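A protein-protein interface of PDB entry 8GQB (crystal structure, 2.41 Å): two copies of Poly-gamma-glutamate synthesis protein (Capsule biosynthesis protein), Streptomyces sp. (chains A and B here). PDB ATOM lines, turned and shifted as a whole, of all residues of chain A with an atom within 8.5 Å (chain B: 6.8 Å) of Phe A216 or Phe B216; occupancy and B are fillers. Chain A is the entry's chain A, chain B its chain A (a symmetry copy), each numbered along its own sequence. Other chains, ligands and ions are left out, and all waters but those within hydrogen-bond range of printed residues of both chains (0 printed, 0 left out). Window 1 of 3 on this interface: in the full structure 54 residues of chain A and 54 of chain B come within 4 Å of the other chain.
O of Phe A216 lies close to O of Phe B216, 2.6 Å away.
The backbone NH (N) of Phe A228 lies close to the backbone carbonyl oxygen (O) of Thr B188 (3.5 Å).
Met A171 touches Leu B190, and with the chains exchanged Leu A190 touches Met B171.
Met A171 touches Phe B216, and with the chains exchanged Phe A216 touches Met B171.
Leu A181 touches Ile B184, and with the chains exchanged Ile A184 touches Leu B181.
Phe A216 touches its own counterpart, Phe B216.
Of the 18 pairs that touch across the chains among the printed residues, 14 have their exchanged pair printed and touching as well.
Hydrophobic or aromatic side chains of chain B within 4 Å of the printed part of chain A: Met B171, Leu B181, Ile B184, Leu B190, Phe B216 and Phe B220.
Of the 24 printed residues of chain A, 10 touch a printed residue of chain B.
Hydrophobic or aromatic side chains of chain A within 4 Å of the printed part of chain B: Met A171, Val A173, Leu A181, Ile A184, Leu A190, Phe A216, Phe A220 and Phe A228.
Among the printed residues, no Asp or Glu carboxylate lies within 4 Å of a Lys or Arg side-chain nitrogen of the other chain.
Among the printed residues, pairs that only touch across the chains: Met A171 with Thr B188 (3.3 Å), Met A171 with Leu B190 (3.8 Å), Met A171 with Phe B216 (3.7 Å), Val A173 with Ile B184 (3.7 Å), Val A173 with Thr B188 (3.9 Å), Leu A181 with Leu B181 (3.7 Å), Leu A181 with Ile B184 (3.9 Å), Ile A184 with Leu B181 (3.9 Å), Thr A188 with Met B171 (3.3 Å), Leu A190 with Met B171 (3.8 Å), Phe A216 with Met B171 (3.7 Å), Phe A216 with Thr B218 (3.4 Å), Phe A216 with Phe B220 (3.99 Å), Thr A218 with Phe B216 (3.4 Å), Phe A220 with Phe B216 (3.99 Å) and Phe A228 with Leu B190 (3.7 Å).
The side-chain hydroxyl of Thr A188 is in hydrogen-bond range of the backbone carbonyl oxygen of Asp A185 (3.4 Å).
The backbone carbonyl oxygen of Asp A185 is in hydrogen-bond range of the backbone NH of Leu A190, 3.3 Å away.
The backbone NH (N) of Phe A220 is in hydrogen-bond range of the backbone carbonyl oxygen (O) of Leu A213 (2.9 Å).
The backbone carbonyl oxygen (O) of Phe A216 sits at hydrogen-bond distance from the side-chain hydroxyl (OG1) of Thr A218.
The backbone NH of Met B171 sits at hydrogen-bond distance from the backbone carbonyl oxygen of Arg B219.
The backbone carbonyl oxygen of Asp B185 lies within hydrogen-bond range of the backbone NH of Leu B190 (3.3 Å).
Of the printed residues of chain B, Leu A181 touches Leu B181 (3.7 Å) and Ile B184 (3.9 Å).
Ala A186 touches none of the printed residues of chain B.
Printed residues of chain B within 4 Å of Phe A216: Met B171, Phe B216, Thr B218 and Phe B220.
Gly A217 touches none of the printed residues of chain B.
Printed residues of chain A within 4 Å of Thr B188: Met A171 (3.3 Å), Val A173 (3.9 Å) and Phe A228 (3.2 Å).
Of the printed residues of chain A, Leu B190 touches Met A171 (3.8 Å) and Phe A228 (3.7 Å).
Of the printed residues of chain A, Phe B216 touches Met A171, Phe A216, Thr A218 and Phe A220.
No residue of chain A comes within 4 Å of Gly B217.
Of the printed residues of chain A, Phe B220 touches Phe A216.
The nearest printed residue of chain A that does not touch Phe B216 is Gly A217 (4.8 Å).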
ATOM      1  N   MET A 171       9.143 -16.575   2.251  1.00  0.00           N
ATOM      2  CA  MET A 171       8.782 -15.246   1.776  1.00  0.00           C
ATOM      3  C   MET A 171       9.613 -14.930   0.538  1.00  0.00           C
ATOM      4  O   MET A 171      10.832 -14.753   0.630  1.00  0.00           O
ATOM      5  CB  MET A 171       9.027 -14.204   2.864  1.00  0.00           C
ATOM      6  CG  MET A 171       8.374 -14.513   4.198  1.00  0.00           C
ATOM      7  SD  MET A 171       6.787 -13.686   4.387  1.00  0.00           S
ATOM      8  CE  MET A 171       7.300 -11.971   4.406  1.00  0.00           C
ATOM      9  N   VAL A 173      10.918 -12.371  -1.983  1.00  0.00           N
ATOM     10  CA  VAL A 173      11.137 -10.935  -2.035  1.00  0.00           C
ATOM     11  C   VAL A 173      12.043 -10.628  -3.217  1.00  0.00           C
ATOM     12  O   VAL A 173      12.804 -11.478  -3.683  1.00  0.00           O
ATOM     13  CB  VAL A 173      11.749 -10.383  -0.727  1.00  0.00           C
ATOM     14  CG1 VAL A 173      10.748 -10.488   0.413  1.00  0.00           C
ATOM     15  CG2 VAL A 173      13.033 -11.128  -0.385  1.00  0.00           C
ATOM     16  N   MET A 178      15.728  -8.023  -0.725  1.00  0.00           N
ATOM     17  CA  MET A 178      16.654  -8.973  -0.114  1.00  0.00           C
ATOM     18  C   MET A 178      17.914  -8.271   0.378  1.00  0.00           C
ATOM     19  O   MET A 178      18.366  -8.496   1.509  1.00  0.00           O
ATOM     20  CB  MET A 178      17.008 -10.070  -1.118  1.00  0.00           C
ATOM     21  CG  MET A 178      18.016 -11.081  -0.602  1.00  0.00           C
ATOM     22  SD  MET A 178      17.323 -12.194   0.632  1.00  0.00           S
ATOM     23  CE  MET A 178      16.595 -13.453  -0.410  1.00  0.00           C
ATOM     24  N   VAL A 180      18.219  -5.136   1.118  1.00  0.00           N
ATOM     25  CA  VAL A 180      17.862  -4.292   2.256  1.00  0.00           C
ATOM     26  C   VAL A 180      17.788  -5.125   3.530  1.00  0.00           C
ATOM     27  O   VAL A 180      18.209  -4.684   4.607  1.00  0.00           O
ATOM     28  CB  VAL A 180      16.545  -3.539   1.991  1.00  0.00           C
ATOM     29  CG1 VAL A 180      16.114  -2.785   3.238  1.00  0.00           C
ATOM     30  CG2 VAL A 180      16.710  -2.569   0.831  1.00  0.00           C
ATOM     31  N   LEU A 181      17.265  -6.349   3.428  1.00  0.00           N
ATOM     32  CA  LEU A 181      17.228  -7.228   4.594  1.00  0.00           C
ATOM     33  C   LEU A 181      18.635  -7.575   5.070  1.00  0.00           C
ATOM     34  O   LEU A 181      18.912  -7.570   6.277  1.00  0.00           O
ATOM     35  CB  LEU A 181      16.437  -8.497   4.271  1.00  0.00           C
ATOM     36  CG  LEU A 181      14.919  -8.331   4.184  1.00  0.00           C
ATOM     37  CD1 LEU A 181      14.278  -9.578   3.598  1.00  0.00           C
ATOM     38  CD2 LEU A 181      14.338  -8.025   5.555  1.00  0.00           C
ATOM     39  N   ARG A 182      19.539  -7.876   4.135  1.00  0.00           N
ATOM     40  CA  ARG A 182      20.919  -8.169   4.517  1.00  0.00           C
ATOM     41  C   ARG A 182      21.578  -6.955   5.162  1.00  0.00           C
ATOM     42  O   ARG A 182      22.347  -7.086   6.124  1.00  0.00           O
ATOM     43  CB  ARG A 182      21.726  -8.625   3.301  1.00  0.00           C
ATOM     44  CG  ARG A 182      21.019  -9.647   2.438  1.00  0.00           C
ATOM     45  CD  ARG A 182      21.909 -10.181   1.333  1.00  0.00           C
ATOM     46  NE  ARG A 182      22.372 -11.535   1.622  1.00  0.00           N
ATOM     47  CZ  ARG A 182      23.148 -12.247   0.813  1.00  0.00           C
ATOM     48  NH1 ARG A 182      23.522 -13.472   1.156  1.00  0.00           N
ATOM     49  NH2 ARG A 182      23.552 -11.734  -0.341  1.00  0.00           N
ATOM     50  N   THR A 183      21.286  -5.761   4.641  1.00  0.00           N
ATOM     51  CA  THR A 183      21.838  -4.539   5.213  1.00  0.00           C
ATOM     52  C   THR A 183      21.310  -4.308   6.624  1.00  0.00           C
ATOM     53  O   THR A 183      22.053  -3.861   7.505  1.00  0.00           O
ATOM     54  CB  THR A 183      21.512  -3.350   4.310  1.00  0.00           C
ATOM     55  OG1 THR A 183      22.025  -3.595   2.994  1.00  0.00           O
ATOM     56  CG2 THR A 183      22.133  -2.074   4.855  1.00  0.00           C
ATOM     57  N   ILE A 184      20.030  -4.605   6.855  1.00  0.00           N
ATOM     58  CA  ILE A 184      19.483  -4.530   8.207  1.00  0.00           C
ATOM     59  C   ILE A 184      20.197  -5.516   9.119  1.00  0.00           C
ATOM     60  O   ILE A 184      20.518  -5.203  10.272  1.00  0.00           O
ATOM     61  CB  ILE A 184      17.962  -4.778   8.187  1.00  0.00           C
ATOM     62  CG1 ILE A 184      17.238  -3.620   7.501  1.00  0.00           C
ATOM     63  CG2 ILE A 184      17.429  -4.984   9.600  1.00  0.00           C
ATOM     64  CD1 ILE A 184      15.739  -3.787   7.458  1.00  0.00           C
ATOM     65  N   ASP A 185      20.460  -6.723   8.614  1.00  0.00           N
ATOM     66  CA  ASP A 185      21.184  -7.720   9.398  1.00  0.00           C
ATOM     67  C   ASP A 185      22.558  -7.205   9.810  1.00  0.00           C
ATOM     68  O   ASP A 185      22.974  -7.359  10.964  1.00  0.00           O
ATOM     69  CB  ASP A 185      21.320  -9.012   8.594  1.00  0.00           C
ATOM     70  CG  ASP A 185      22.125 -10.071   9.320  1.00  0.00           C
ATOM     71  OD1 ASP A 185      21.717 -10.473  10.429  1.00  0.00           O
ATOM     72  OD2 ASP A 185      23.164 -10.505   8.778  1.00  0.00           O
ATOM     73  N   ALA A 186      23.277  -6.588   8.872  1.00  0.00           N
ATOM     74  CA  ALA A 186      24.648  -6.169   9.152  1.00  0.00           C
ATOM     75  C   ALA A 186      24.689  -4.932  10.043  1.00  0.00           C
ATOM     76  O   ALA A 186      25.410  -4.902  11.047  1.00  0.00           O
ATOM     77  CB  ALA A 186      25.396  -5.917   7.843  1.00  0.00           C
ATOM     78  N   THR A 188      22.509  -3.461  12.066  1.00  0.00           N
ATOM     79  CA  THR A 188      21.957  -3.519  13.415  1.00  0.00           C
ATOM     80  C   THR A 188      22.875  -4.234  14.396  1.00  0.00           C
ATOM     81  O   THR A 188      22.679  -4.110  15.610  1.00  0.00           O
ATOM     82  CB  THR A 188      20.593  -4.214  13.412  1.00  0.00           C
ATOM     83  OG1 THR A 188      20.707  -5.492  12.773  1.00  0.00           O
ATOM     84  CG2 THR A 188      19.557  -3.368  12.685  1.00  0.00           C
ATOM     85  N   LEU A 190      23.132  -7.586  14.302  1.00  0.00           N
ATOM     86  CA  LEU A 190      22.617  -8.941  14.461  1.00  0.00           C
ATOM     87  C   LEU A 190      23.595  -9.968  13.908  1.00  0.00           C
ATOM     88  O   LEU A 190      23.789 -11.033  14.507  1.00  0.00           O
ATOM     89  CB  LEU A 190      21.262  -9.073  13.769  1.00  0.00           C
ATOM     90  CG  LEU A 190      20.525 -10.396  13.982  1.00  0.00           C
ATOM     91  CD1 LEU A 190      19.884 -10.433  15.363  1.00  0.00           C
ATOM     92  CD2 LEU A 190      19.490 -10.629  12.889  1.00  0.00           C
ATOM     93  N   ARG A 191      24.212  -9.666  12.763  1.00  0.00           N
ATOM     94  CA  ARG A 191      25.193 -10.573  12.177  1.00  0.00           C
ATOM     95  C   ARG A 191      26.361 -10.807  13.123  1.00  0.00           C
ATOM     96  O   ARG A 191      26.838 -11.940  13.260  1.00  0.00           O
ATOM     97  CB  ARG A 191      25.691 -10.017  10.844  1.00  0.00           C
ATOM     98  CG  ARG A 191      26.539 -10.978  10.026  1.00  0.00           C
ATOM     99  CD  ARG A 191      27.089 -10.275   8.793  1.00  0.00           C
ATOM    100  NE  ARG A 191      27.944  -9.147   9.155  1.00  0.00           N
ATOM    101  CZ  ARG A 191      28.428  -8.260   8.289  1.00  0.00           C
ATOM    102  NH1 ARG A 191      28.138  -8.361   6.999  1.00  0.00           N
ATOM    103  NH2 ARG A 191      29.202  -7.269   8.714  1.00  0.00           N
ATOM    104  N   ARG A 194      26.204 -13.637  15.553  1.00  0.00           N
ATOM    105  CA  ARG A 194      26.370 -15.001  15.073  1.00  0.00           C
ATOM    106  C   ARG A 194      27.836 -15.396  14.959  1.00  0.00           C
ATOM    107  O   ARG A 194      28.133 -16.518  14.532  1.00  0.00           O
ATOM    108  CB  ARG A 194      25.665 -15.185  13.727  1.00  0.00           C
ATOM    109  CG  ARG A 194      24.166 -14.955  13.792  1.00  0.00           C
ATOM    110  CD  ARG A 194      23.446 -15.471  12.554  1.00  0.00           C
ATOM    111  NE  ARG A 194      23.938 -14.847  11.330  1.00  0.00           N
ATOM    112  CZ  ARG A 194      23.447 -13.727  10.810  1.00  0.00           C
ATOM    113  NH1 ARG A 194      22.442 -13.099  11.407  1.00  0.00           N
ATOM    114  NH2 ARG A 194      23.964 -13.233   9.693  1.00  0.00           N
ATOM    115  N   ALA A 206      22.918 -18.299   8.424  1.00  0.00           N
ATOM    116  CA  ALA A 206      21.928 -17.456   7.769  1.00  0.00           C
ATOM    117  C   ALA A 206      22.062 -17.446   6.254  1.00  0.00           C
ATOM    118  O   ALA A 206      21.128 -17.016   5.567  1.00  0.00           O
ATOM    119  CB  ALA A 206      22.027 -16.020   8.296  1.00  0.00           C
ATOM    120  N   LEU A 213      18.119 -16.952   2.084  1.00  0.00           N
ATOM    121  CA  LEU A 213      18.526 -16.289   3.314  1.00  0.00           C
ATOM    122  C   LEU A 213      17.626 -16.766   4.444  1.00  0.00           C
ATOM    123  O   LEU A 213      16.494 -17.189   4.213  1.00  0.00           O
ATOM    124  CB  LEU A 213      18.451 -14.765   3.170  1.00  0.00           C
ATOM    125  CG  LEU A 213      19.613 -13.944   3.720  1.00  0.00           C
ATOM    126  CD1 LEU A 213      20.920 -14.345   3.065  1.00  0.00           C
ATOM    127  CD2 LEU A 213      19.338 -12.475   3.500  1.00  0.00           C
ATOM    128  N   ALA A 214      18.138 -16.681   5.670  1.00  0.00           N
ATOM    129  CA  ALA A 214      17.388 -17.101   6.852  1.00  0.00           C
ATOM    130  C   ALA A 214      17.687 -16.134   7.990  1.00  0.00           C
ATOM    131  O   ALA A 214      18.793 -16.142   8.541  1.00  0.00           O
ATOM    132  CB  ALA A 214      17.737 -18.535   7.249  1.00  0.00           C
ATOM    133  N   LEU A 215      16.706 -15.302   8.338  1.00  0.00           N
ATOM    134  CA  LEU A 215      16.867 -14.343   9.423  1.00  0.00           C
ATOM    135  C   LEU A 215      15.535 -14.168  10.131  1.00  0.00           C
ATOM    136  O   LEU A 215      14.467 -14.377   9.550  1.00  0.00           O
ATOM    137  CB  LEU A 215      17.365 -12.973   8.941  1.00  0.00           C
ATOM    138  CG  LEU A 215      18.313 -12.833   7.754  1.00  0.00           C
ATOM    139  CD1 LEU A 215      17.529 -12.908   6.461  1.00  0.00           C
ATOM    140  CD2 LEU A 215      19.045 -11.517   7.851  1.00  0.00           C
ATOM    141  N   PHE A 216      15.617 -13.754  11.395  1.00  0.00           N
ATOM    142  CA  PHE A 216      14.441 -13.530  12.232  1.00  0.00           C
ATOM    143  C   PHE A 216      13.561 -14.774  12.304  1.00  0.00           C
ATOM    144  O   PHE A 216      12.337 -14.678  12.382  1.00  0.00           O
ATOM    145  CB  PHE A 216      13.626 -12.328  11.738  1.00  0.00           C
ATOM    146  CG  PHE A 216      14.452 -11.259  11.072  1.00  0.00           C
ATOM    147  CD1 PHE A 216      15.329 -10.479  11.808  1.00  0.00           C
ATOM    148  CD2 PHE A 216      14.334 -11.022   9.711  1.00  0.00           C
ATOM    149  CE1 PHE A 216      16.082  -9.493  11.197  1.00  0.00           C
ATOM    150  CE2 PHE A 216      15.084 -10.036   9.095  1.00  0.00           C
ATOM    151  CZ  PHE A 216      15.959  -9.270   9.840  1.00  0.00           C
ATOM    152  N   GLY A 217      14.172 -15.955  12.264  1.00  0.00           N
ATOM    153  CA  GLY A 217      13.398 -17.185  12.272  1.00  0.00           C
ATOM    154  C   GLY A 217      12.491 -17.345  11.073  1.00  0.00           C
ATOM    155  O   GLY A 217      11.461 -18.022  11.166  1.00  0.00           O
ATOM    156  N   THR A 218      12.845 -16.732   9.946  1.00  0.00           N
ATOM    157  CA  THR A 218      12.058 -16.798   8.724  1.00  0.00           C
ATOM    158  C   THR A 218      13.004 -16.904   7.540  1.00  0.00           C
ATOM    159  O   THR A 218      14.062 -16.264   7.523  1.00  0.00           O
ATOM    160  CB  THR A 218      11.153 -15.564   8.567  1.00  0.00           C
ATOM    161  OG1 THR A 218      10.421 -15.347   9.781  1.00  0.00           O
ATOM    162  CG2 THR A 218      10.170 -15.759   7.419  1.00  0.00           C
ATOM    163  N   ARG A 219      12.626 -17.710   6.552  1.00  0.00           N
ATOM    164  CA  ARG A 219      13.446 -17.924   5.369  1.00  0.00           C
ATOM    165  C   ARG A 219      12.929 -17.079   4.211  1.00  0.00           C
ATOM    166  O   ARG A 219      11.738 -17.121   3.882  1.00  0.00           O
ATOM    167  CB  ARG A 219      13.480 -19.405   4.983  1.00  0.00           C
ATOM    168  CG  ARG A 219      12.125 -20.090   4.939  1.00  0.00           C
ATOM    169  CD  ARG A 219      12.268 -21.526   4.459  1.00  0.00           C
ATOM    170  NE  ARG A 219      12.945 -22.372   5.439  1.00  0.00           N
ATOM    171  CZ  ARG A 219      13.612 -23.480   5.134  1.00  0.00           C
ATOM    172  NH1 ARG A 219      13.708 -23.872   3.871  1.00  0.00           N
ATOM    173  NH2 ARG A 219      14.195 -24.191   6.090  1.00  0.00           N
ATOM    174  N   PHE A 220      13.829 -16.310   3.606  1.00  0.00           N
ATOM    175  CA  PHE A 220      13.538 -15.471   2.456  1.00  0.00           C
ATOM    176  C   PHE A 220      14.256 -16.015   1.227  1.00  0.00           C
ATOM    177  O   PHE A 220      15.313 -16.646   1.333  1.00  0.00           O
ATOM    178  CB  PHE A 220      13.972 -14.021   2.702  1.00  0.00           C
ATOM    179  CG  PHE A 220      13.316 -13.377   3.891  1.00  0.00           C
ATOM    180  CD1 PHE A 220      13.862 -13.508   5.157  1.00  0.00           C
ATOM    181  CD2 PHE A 220      12.160 -12.629   3.739  1.00  0.00           C
ATOM    182  CE1 PHE A 220      13.262 -12.913   6.251  1.00  0.00           C
ATOM    183  CE2 PHE A 220      11.556 -12.030   4.830  1.00  0.00           C
ATOM    184  CZ  PHE A 220      12.108 -12.173   6.087  1.00  0.00           C
ATOM    185  N   PHE A 228       4.450 -15.496  -1.264  1.00  0.00           N
ATOM    186  CA  PHE A 228       4.437 -16.271  -0.028  1.00  0.00           C
ATOM    187  C   PHE A 228       4.065 -17.701  -0.375  1.00  0.00           C
ATOM    188  O   PHE A 228       2.988 -17.935  -0.933  1.00  0.00           O
ATOM    189  CB  PHE A 228       3.439 -15.673   0.967  1.00  0.00           C
ATOM    190  CG  PHE A 228       3.431 -16.347   2.306  1.00  0.00           C
ATOM    191  CD1 PHE A 228       2.618 -17.442   2.541  1.00  0.00           C
ATOM    192  CD2 PHE A 228       4.221 -15.871   3.336  1.00  0.00           C
ATOM    193  CE1 PHE A 228       2.604 -18.059   3.774  1.00  0.00           C
ATOM    194  CE2 PHE A 228       4.211 -16.482   4.573  1.00  0.00           C
ATOM    195  CZ  PHE A 228       3.401 -17.577   4.793  1.00  0.00           C
ATOM    196  N   MET B 171      15.341  -4.708  17.464  1.00  0.00           N
ATOM    197  CA  MET B 171      16.186  -4.268  16.361  1.00  0.00           C
ATOM    198  C   MET B 171      15.837  -2.822  16.028  1.00  0.00           C
ATOM    199  O   MET B 171      14.743  -2.541  15.528  1.00  0.00           O
ATOM    200  CB  MET B 171      15.982  -5.162  15.140  1.00  0.00           C
ATOM    201  CG  MET B 171      16.144  -6.646  15.406  1.00  0.00           C
ATOM    202  SD  MET B 171      17.797  -7.233  15.003  1.00  0.00           S
ATOM    203  CE  MET B 171      17.822  -6.981  13.230  1.00  0.00           C
ATOM    204  N   LEU B 181      10.553  -2.741   5.417  1.00  0.00           N
ATOM    205  CA  LEU B 181      10.027  -3.925   6.090  1.00  0.00           C
ATOM    206  C   LEU B 181       8.507  -3.992   5.982  1.00  0.00           C
ATOM    207  O   LEU B 181       7.938  -5.062   5.724  1.00  0.00           O
ATOM    208  CB  LEU B 181      10.467  -3.937   7.554  1.00  0.00           C
ATOM    209  CG  LEU B 181      11.935  -4.287   7.806  1.00  0.00           C
ATOM    210  CD1 LEU B 181      12.313  -4.003   9.249  1.00  0.00           C
ATOM    211  CD2 LEU B 181      12.201  -5.743   7.460  1.00  0.00           C
ATOM    212  N   ILE B 184       7.627  -5.079   2.519  1.00  0.00           N
ATOM    213  CA  ILE B 184       7.800  -6.523   2.387  1.00  0.00           C
ATOM    214  C   ILE B 184       6.616  -7.253   3.005  1.00  0.00           C
ATOM    215  O   ILE B 184       6.112  -8.236   2.450  1.00  0.00           O
ATOM    216  CB  ILE B 184       9.131  -6.967   3.024  1.00  0.00           C
ATOM    217  CG1 ILE B 184      10.315  -6.443   2.211  1.00  0.00           C
ATOM    218  CG2 ILE B 184       9.192  -8.484   3.147  1.00  0.00           C
ATOM    219  CD1 ILE B 184      11.656  -6.852   2.767  1.00  0.00           C
ATOM    220  N   ASP B 185       6.152  -6.778   4.163  1.00  0.00           N
ATOM    221  CA  ASP B 185       4.990  -7.384   4.807  1.00  0.00           C
ATOM    222  C   ASP B 185       3.770  -7.339   3.897  1.00  0.00           C
ATOM    223  O   ASP B 185       3.041  -8.329   3.762  1.00  0.00           O
ATOM    224  CB  ASP B 185       4.697  -6.668   6.125  1.00  0.00           C
ATOM    225  CG  ASP B 185       3.457  -7.199   6.816  1.00  0.00           C
ATOM    226  OD1 ASP B 185       3.426  -8.403   7.140  1.00  0.00           O
ATOM    227  OD2 ASP B 185       2.516  -6.408   7.040  1.00  0.00           O
ATOM    228  N   THR B 188       4.322  -9.244   0.001  1.00  0.00           N
ATOM    229  CA  THR B 188       4.461 -10.696  -0.002  1.00  0.00           C
ATOM    230  C   THR B 188       3.151 -11.412   0.293  1.00  0.00           C
ATOM    231  O   THR B 188       3.051 -12.619   0.044  1.00  0.00           O
ATOM    232  CB  THR B 188       5.513 -11.140   1.017  1.00  0.00           C
ATOM    233  OG1 THR B 188       5.201 -10.587   2.302  1.00  0.00           O
ATOM    234  CG2 THR B 188       6.904 -10.691   0.589  1.00  0.00           C
ATOM    235  N   LEU B 190       1.959 -11.482   3.437  1.00  0.00           N
ATOM    236  CA  LEU B 190       1.994 -11.879   4.840  1.00  0.00           C
ATOM    237  C   LEU B 190       0.938 -11.137   5.647  1.00  0.00           C
ATOM    238  O   LEU B 190       0.292 -11.725   6.523  1.00  0.00           O
ATOM    239  CB  LEU B 190       3.383 -11.624   5.423  1.00  0.00           C
ATOM    240  CG  LEU B 190       3.619 -12.136   6.845  1.00  0.00           C
ATOM    241  CD1 LEU B 190       3.837 -13.643   6.841  1.00  0.00           C
ATOM    242  CD2 LEU B 190       4.787 -11.412   7.501  1.00  0.00           C
ATOM    243  N   ALA B 214       6.143  -5.346  14.707  1.00  0.00           N
ATOM    244  CA  ALA B 214       6.402  -6.722  15.126  1.00  0.00           C
ATOM    245  C   ALA B 214       6.114  -7.652  13.955  1.00  0.00           C
ATOM    246  O   ALA B 214       4.950  -7.854  13.591  1.00  0.00           O
ATOM    247  CB  ALA B 214       5.558  -7.098  16.343  1.00  0.00           C
ATOM    248  N   LEU B 215       7.169  -8.213  13.365  1.00  0.00           N
ATOM    249  CA  LEU B 215       7.018  -9.133  12.246  1.00  0.00           C
ATOM    250  C   LEU B 215       8.110 -10.186  12.320  1.00  0.00           C
ATOM    251  O   LEU B 215       9.183  -9.959  12.886  1.00  0.00           O
ATOM    252  CB  LEU B 215       7.086  -8.432  10.882  1.00  0.00           C
ATOM    253  CG  LEU B 215       6.565  -7.013  10.679  1.00  0.00           C
ATOM    254  CD1 LEU B 215       7.601  -6.015  11.149  1.00  0.00           C
ATOM    255  CD2 LEU B 215       6.251  -6.800   9.218  1.00  0.00           C
ATOM    256  N   PHE B 216       7.826 -11.339  11.715  1.00  0.00           N
ATOM    257  CA  PHE B 216       8.756 -12.465  11.682  1.00  0.00           C
ATOM    258  C   PHE B 216       9.182 -12.878  13.088  1.00  0.00           C
ATOM    259  O   PHE B 216      10.316 -13.304  13.303  1.00  0.00           O
ATOM    260  CB  PHE B 216       9.985 -12.148  10.823  1.00  0.00           C
ATOM    261  CG  PHE B 216       9.713 -11.197   9.687  1.00  0.00           C
ATOM    262  CD1 PHE B 216       8.942 -11.588   8.605  1.00  0.00           C
ATOM    263  CD2 PHE B 216      10.245  -9.917   9.696  1.00  0.00           C
ATOM    264  CE1 PHE B 216       8.696 -10.716   7.559  1.00  0.00           C
ATOM    265  CE2 PHE B 216      10.003  -9.041   8.652  1.00  0.00           C
ATOM    266  CZ  PHE B 216       9.228  -9.442   7.582  1.00  0.00           C
ATOM    267  N   GLY B 217       8.285 -12.743  14.061  1.00  0.00           N
ATOM    268  CA  GLY B 217       8.634 -13.064  15.435  1.00  0.00           C
ATOM    269  C   GLY B 217       9.735 -12.196  16.003  1.00  0.00           C
ATOM    270  O   GLY B 217      10.461 -12.634  16.903  1.00  0.00           O
ATOM    271  N   THR B 218       9.883 -10.976  15.495  1.00  0.00           N
ATOM    272  CA  THR B 218      10.907 -10.045  15.946  1.00  0.00           C
ATOM    273  C   THR B 218      10.314  -8.646  15.978  1.00  0.00           C
ATOM    274  O   THR B 218       9.532  -8.276  15.094  1.00  0.00           O
ATOM    275  CB  THR B 218      12.141 -10.074  15.029  1.00  0.00           C
ATOM    276  OG1 THR B 218      12.561 -11.430  14.830  1.00  0.00           O
ATOM    277  CG2 THR B 218      13.288  -9.280  15.644  1.00  0.00           C
ATOM    278  N   ARG B 219      10.683  -7.871  16.993  1.00  0.00           N
ATOM    279  CA  ARG B 219      10.175  -6.518  17.160  1.00  0.00           C
ATOM    280  C   ARG B 219      11.200  -5.506  16.663  1.00  0.00           C
ATOM    281  O   ARG B 219      12.369  -5.543  17.063  1.00  0.00           O
ATOM    282  CB  ARG B 219       9.811  -6.244  18.622  1.00  0.00           C
ATOM    283  CG  ARG B 219      10.869  -6.645  19.635  1.00  0.00           C
ATOM    284  CD  ARG B 219      10.442  -6.246  21.040  1.00  0.00           C
ATOM    285  NE  ARG B 219       9.316  -7.042  21.523  1.00  0.00           N
ATOM    286  CZ  ARG B 219       8.458  -6.633  22.451  1.00  0.00           C
ATOM    287  NH1 ARG B 219       8.584  -5.428  22.989  1.00  0.00           N
ATOM    288  NH2 ARG B 219       7.464  -7.424  22.834  1.00  0.00           N
ATOM    289  N   PHE B 220      10.755  -4.611  15.786  1.00  0.00           N
ATOM    290  CA  PHE B 220      11.568  -3.541  15.234  1.00  0.00           C
ATOM    291  C   PHE B 220      11.068  -2.197  15.750  1.00  0.00           C
ATOM    292  O   PHE B 220       9.884  -2.033  16.060  1.00  0.00           O
ATOM    293  CB  PHE B 220      11.528  -3.548  13.701  1.00  0.00           C
ATOM    294  CG  PHE B 220      12.010  -4.829  13.080  1.00  0.00           C
ATOM    295  CD1 PHE B 220      11.140  -5.886  12.872  1.00  0.00           C
ATOM    296  CD2 PHE B 220      13.332  -4.970  12.690  1.00  0.00           C
ATOM    297  CE1 PHE B 220      11.580  -7.063  12.298  1.00  0.00           C
ATOM    298  CE2 PHE B 220      13.779  -6.145  12.114  1.00  0.00           C
ATOM    299  CZ  PHE B 220      12.901  -7.192  11.918  1.00  0.00           C
